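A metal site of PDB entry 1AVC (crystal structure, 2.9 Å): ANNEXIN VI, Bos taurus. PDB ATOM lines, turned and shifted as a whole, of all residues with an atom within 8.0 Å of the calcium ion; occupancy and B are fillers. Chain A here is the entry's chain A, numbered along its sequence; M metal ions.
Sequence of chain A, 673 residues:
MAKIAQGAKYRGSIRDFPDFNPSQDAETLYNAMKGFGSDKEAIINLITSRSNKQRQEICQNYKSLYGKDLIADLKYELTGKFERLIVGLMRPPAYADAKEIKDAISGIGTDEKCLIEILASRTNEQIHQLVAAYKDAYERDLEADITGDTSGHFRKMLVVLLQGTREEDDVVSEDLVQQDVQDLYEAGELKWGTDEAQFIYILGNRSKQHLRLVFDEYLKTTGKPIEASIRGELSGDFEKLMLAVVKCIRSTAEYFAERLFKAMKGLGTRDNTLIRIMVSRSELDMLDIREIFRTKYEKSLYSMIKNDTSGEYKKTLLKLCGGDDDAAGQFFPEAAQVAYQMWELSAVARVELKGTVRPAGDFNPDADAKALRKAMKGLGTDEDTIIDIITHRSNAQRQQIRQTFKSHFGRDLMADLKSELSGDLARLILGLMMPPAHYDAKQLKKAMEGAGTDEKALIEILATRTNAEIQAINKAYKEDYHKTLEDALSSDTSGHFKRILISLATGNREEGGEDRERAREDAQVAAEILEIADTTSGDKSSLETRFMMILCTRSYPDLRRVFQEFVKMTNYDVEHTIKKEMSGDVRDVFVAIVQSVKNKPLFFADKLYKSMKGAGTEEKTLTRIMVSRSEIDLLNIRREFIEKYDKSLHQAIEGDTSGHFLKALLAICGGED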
ATOM      1  N   PHE A 261     -15.231 -18.646 -27.615  1.00  0.00           N
ATOM      2  CA  PHE A 261     -13.989 -18.705 -26.863  1.00  0.00           C
ATOM      3  C   PHE A 261     -12.822 -18.323 -27.773  1.00  0.00           C
ATOM      4  O   PHE A 261     -11.920 -17.584 -27.371  1.00  0.00           O
ATOM      5  CB  PHE A 261     -13.777 -20.118 -26.315  1.00  0.00           C
ATOM      6  CG  PHE A 261     -12.490 -20.288 -25.548  1.00  0.00           C
ATOM      7  CD1 PHE A 261     -11.325 -20.686 -26.206  1.00  0.00           C
ATOM      8  CD2 PHE A 261     -12.446 -20.079 -24.172  1.00  0.00           C
ATOM      9  CE1 PHE A 261     -10.141 -20.865 -25.500  1.00  0.00           C
ATOM     10  CE2 PHE A 261     -11.262 -20.258 -23.467  1.00  0.00           C
ATOM     11  CZ  PHE A 261     -10.110 -20.650 -24.125  1.00  0.00           C
ATOM     12  N   LYS A 262     -12.867 -18.819 -29.010  1.00  0.00           N
ATOM     13  CA  LYS A 262     -11.824 -18.550 -29.998  1.00  0.00           C
ATOM     14  C   LYS A 262     -11.728 -17.068 -30.360  1.00  0.00           C
ATOM     15  O   LYS A 262     -10.626 -16.551 -30.582  1.00  0.00           O
ATOM     16  CB  LYS A 262     -12.095 -19.365 -31.268  1.00  0.00           C
ATOM     17  CG  LYS A 262     -11.239 -20.614 -31.397  1.00  0.00           C
ATOM     18  CD  LYS A 262     -12.028 -21.855 -31.006  1.00  0.00           C
ATOM     19  CE  LYS A 262     -11.212 -23.117 -31.214  1.00  0.00           C
ATOM     20  NZ  LYS A 262     -11.153 -23.493 -32.657  1.00  0.00           N
ATOM     21  N   ALA A 263     -12.869 -16.399 -30.422  1.00  0.00           N
ATOM     22  CA  ALA A 263     -12.910 -14.980 -30.778  1.00  0.00           C
ATOM     23  C   ALA A 263     -12.381 -14.065 -29.678  1.00  0.00           C
ATOM     24  O   ALA A 263     -12.090 -12.897 -29.926  1.00  0.00           O
ATOM     25  CB  ALA A 263     -14.330 -14.587 -31.142  1.00  0.00           C
ATOM     26  N   MET A 264     -12.249 -14.591 -28.469  1.00  0.00           N
ATOM     27  CA  MET A 264     -11.751 -13.808 -27.343  1.00  0.00           C
ATOM     28  C   MET A 264     -10.406 -14.321 -26.833  1.00  0.00           C
ATOM     29  O   MET A 264      -9.750 -13.670 -26.031  1.00  0.00           O
ATOM     30  CB  MET A 264     -12.777 -13.819 -26.207  1.00  0.00           C
ATOM     31  CG  MET A 264     -14.200 -13.525 -26.669  1.00  0.00           C
ATOM     32  SD  MET A 264     -15.282 -12.998 -25.321  1.00  0.00           S
ATOM     33  CE  MET A 264     -16.342 -14.430 -25.171  1.00  0.00           C
ATOM     34  N   LYS A 265     -10.001 -15.495 -27.311  1.00  0.00           N
ATOM     35  CA  LYS A 265      -8.751 -16.112 -26.880  1.00  0.00           C
ATOM     36  C   LYS A 265      -7.547 -15.228 -27.209  1.00  0.00           C
ATOM     37  O   LYS A 265      -7.415 -14.733 -28.320  1.00  0.00           O
ATOM     38  CB  LYS A 265      -8.597 -17.475 -27.559  1.00  0.00           C
ATOM     39  CG  LYS A 265      -7.208 -17.776 -28.095  1.00  0.00           C
ATOM     40  CD  LYS A 265      -7.273 -18.679 -29.320  1.00  0.00           C
ATOM     41  CE  LYS A 265      -7.531 -17.884 -30.587  1.00  0.00           C
ATOM     42  NZ  LYS A 265      -8.006 -18.742 -31.703  1.00  0.00           N
ATOM     43  N   GLY A 266      -6.665 -15.051 -26.221  1.00  0.00           N
ATOM     44  CA  GLY A 266      -5.467 -14.236 -26.410  1.00  0.00           C
ATOM     45  C   GLY A 266      -5.758 -12.785 -26.732  1.00  0.00           C
ATOM     46  O   GLY A 266      -6.783 -12.469 -27.333  1.00  0.00           O
ATOM     47  N   LEU A 267      -4.844 -11.886 -26.341  1.00  0.00           N
ATOM     48  CA  LEU A 267      -5.013 -10.453 -26.610  1.00  0.00           C
ATOM     49  C   LEU A 267      -5.611 -10.192 -27.993  1.00  0.00           C
ATOM     50  O   LEU A 267      -5.278 -10.872 -28.959  1.00  0.00           O
ATOM     51  CB  LEU A 267      -3.661  -9.738 -26.491  1.00  0.00           C
ATOM     52  CG  LEU A 267      -3.252  -9.284 -25.081  1.00  0.00           C
ATOM     53  CD1 LEU A 267      -3.170 -10.486 -24.148  1.00  0.00           C
ATOM     54  CD2 LEU A 267      -1.919  -8.558 -25.156  1.00  0.00           C
ATOM     55  N   GLY A 268      -6.497  -9.204 -28.083  1.00  0.00           N
ATOM     56  CA  GLY A 268      -7.128  -8.896 -29.353  1.00  0.00           C
ATOM     57  C   GLY A 268      -8.386  -9.714 -29.517  1.00  0.00           C
ATOM     58  O   GLY A 268      -8.393 -10.920 -29.271  1.00  0.00           O
ATOM     59  N   THR A 269      -9.468  -9.064 -29.940  1.00  0.00           N
ATOM     60  CA  THR A 269     -10.743  -9.762 -30.110  1.00  0.00           C
ATOM     61  C   THR A 269     -11.238  -9.772 -31.548  1.00  0.00           C
ATOM     62  O   THR A 269     -11.027  -8.824 -32.303  1.00  0.00           O
ATOM     63  CB  THR A 269     -11.822  -9.117 -29.231  1.00  0.00           C
ATOM     64  OG1 THR A 269     -11.366  -9.057 -27.881  1.00  0.00           O
ATOM     65  CG2 THR A 269     -13.123  -9.922 -29.277  1.00  0.00           C
ATOM     66  N   ARG A 270     -11.905 -10.857 -31.932  1.00  0.00           N
ATOM     67  CA  ARG A 270     -12.480 -10.973 -33.266  1.00  0.00           C
ATOM     68  C   ARG A 270     -13.918 -10.479 -33.149  1.00  0.00           C
ATOM     69  O   ARG A 270     -14.863 -11.203 -33.422  1.00  0.00           O
ATOM     70  CB  ARG A 270     -12.454 -12.442 -33.721  1.00  0.00           C
ATOM     71  CG  ARG A 270     -11.229 -12.813 -34.553  1.00  0.00           C
ATOM     72  CD  ARG A 270      -9.932 -12.608 -33.774  1.00  0.00           C
ATOM     73  NE  ARG A 270      -9.932 -13.347 -32.509  1.00  0.00           N
ATOM     74  CZ  ARG A 270      -8.931 -13.329 -31.640  1.00  0.00           C
ATOM     75  NH1 ARG A 270      -7.838 -12.617 -31.887  1.00  0.00           N
ATOM     76  NH2 ARG A 270      -9.010 -14.027 -30.512  1.00  0.00           N
ATOM     77  N   ASP A 271     -14.045  -9.225 -32.718  1.00  0.00           N
ATOM     78  CA  ASP A 271     -15.340  -8.580 -32.518  1.00  0.00           C
ATOM     79  C   ASP A 271     -16.408  -8.905 -33.550  1.00  0.00           C
ATOM     80  O   ASP A 271     -17.566  -9.126 -33.196  1.00  0.00           O
ATOM     81  CB  ASP A 271     -15.140  -7.063 -32.469  1.00  0.00           C
ATOM     82  CG  ASP A 271     -13.903  -6.665 -31.686  1.00  0.00           C
ATOM     83  OD1 ASP A 271     -13.988  -6.556 -30.440  1.00  0.00           O
ATOM     84  OD2 ASP A 271     -12.841  -6.457 -32.312  1.00  0.00           O
ATOM     85  N   MET A 304     -15.434 -13.692 -19.646  1.00  0.00           N
ATOM     86  CA  MET A 304     -14.567 -13.544 -20.813  1.00  0.00           C
ATOM     87  C   MET A 304     -14.914 -12.291 -21.615  1.00  0.00           C
ATOM     88  O   MET A 304     -14.021 -11.562 -22.049  1.00  0.00           O
ATOM     89  CB  MET A 304     -14.679 -14.777 -21.714  1.00  0.00           C
ATOM     90  CG  MET A 304     -13.654 -14.797 -22.846  1.00  0.00           C
ATOM     91  SD  MET A 304     -12.772 -16.373 -23.033  1.00  0.00           S
ATOM     92  CE  MET A 304     -12.626 -16.902 -21.329  1.00  0.00           C
ATOM     93  N   ASN A 307     -14.024  -8.934 -19.777  1.00  0.00           N
ATOM     94  CA  ASN A 307     -12.592  -8.620 -19.767  1.00  0.00           C
ATOM     95  C   ASN A 307     -12.016  -8.296 -21.141  1.00  0.00           C
ATOM     96  O   ASN A 307     -10.987  -7.639 -21.252  1.00  0.00           O
ATOM     97  CB  ASN A 307     -11.807  -9.783 -19.161  1.00  0.00           C
ATOM     98  CG  ASN A 307     -12.229 -10.094 -17.735  1.00  0.00           C
ATOM     99  OD1 ASN A 307     -12.039 -11.205 -17.246  1.00  0.00           O
ATOM    100  ND2 ASN A 307     -12.811  -9.108 -17.055  1.00  0.00           N
ATOM    101  N   ASP A 308     -12.686  -8.753 -22.191  1.00  0.00           N
ATOM    102  CA  ASP A 308     -12.200  -8.507 -23.547  1.00  0.00           C
ATOM    103  C   ASP A 308     -12.777  -7.280 -24.238  1.00  0.00           C
ATOM    104  O   ASP A 308     -12.167  -6.725 -25.158  1.00  0.00           O
ATOM    105  CB  ASP A 308     -12.458  -9.739 -24.410  1.00  0.00           C
ATOM    106  CG  ASP A 308     -11.212 -10.232 -25.095  1.00  0.00           C
ATOM    107  OD1 ASP A 308     -10.101 -10.023 -24.561  1.00  0.00           O
ATOM    108  OD2 ASP A 308     -11.338 -10.828 -26.179  1.00  0.00           O
ATOM    109  N   THR A 309     -13.957  -6.853 -23.807  1.00  0.00           N
ATOM    110  CA  THR A 309     -14.596  -5.685 -24.400  1.00  0.00           C
ATOM    111  C   THR A 309     -14.712  -4.522 -23.413  1.00  0.00           C
ATOM    112  O   THR A 309     -14.473  -4.689 -22.218  1.00  0.00           O
ATOM    113  CB  THR A 309     -15.998  -6.039 -24.940  1.00  0.00           C
ATOM    114  OG1 THR A 309     -16.813  -6.532 -23.869  1.00  0.00           O
ATOM    115  CG2 THR A 309     -15.904  -7.105 -26.021  1.00  0.00           C
ATOM    116  N   TYR A 609      -0.386 -23.198 -22.556  1.00  0.00           N
ATOM    117  CA  TYR A 609      -0.895 -21.941 -23.099  1.00  0.00           C
ATOM    118  C   TYR A 609      -0.775 -20.825 -22.071  1.00  0.00           C
ATOM    119  O   TYR A 609      -0.329 -19.724 -22.389  1.00  0.00           O
ATOM    120  CB  TYR A 609      -2.365 -22.097 -23.503  1.00  0.00           C
ATOM    121  CG  TYR A 609      -2.952 -20.867 -24.145  1.00  0.00           C
ATOM    122  CD1 TYR A 609      -2.757 -20.596 -25.498  1.00  0.00           C
ATOM    123  CD2 TYR A 609      -3.698 -19.955 -23.396  1.00  0.00           C
ATOM    124  CE1 TYR A 609      -3.292 -19.460 -26.096  1.00  0.00           C
ATOM    125  CE2 TYR A 609      -4.237 -18.807 -23.976  1.00  0.00           C
ATOM    126  CZ  TYR A 609      -4.033 -18.564 -25.325  1.00  0.00           C
ATOM    127  OH  TYR A 609      -4.565 -17.436 -25.912  1.00  0.00           O
HETATM  128 CA    CA M   1      -8.807 -11.255 -26.622  1.00  0.00          CA
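N of Gly 266 is in hydrogen-bond range of OH of Tyr 609 (3.2 Å).
OG1 of Thr 269 sits close to OD2 of Asp 308.
The backbone carbonyl oxygen (O) of Gly 268 lies close to the guanidinium group (NH1) of Arg 270, at 3.2 Å.
C of Leu 267 touches the calcium ion (3.6 Å).
Thr 269 touches the calcium ion (OG1 to CA, 3.6 Å).
Of the 16 residues printed, 6 come within 4 Å of the calcium ion.
O of Gly 266 binds the calcium ion (2.5 Å).
The calcium ion is bound by OD2 of Asp 308.
O of Met 264 is bound to the calcium ion (2.7 Å).
The calcium ion is bound by O of Gly 268 (2.7 Å).
The side-chain carboxylate (OD1) of Asp 308 binds the calcium ion (2.7 Å).
The calcium ion has five donor atoms within binding distance.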
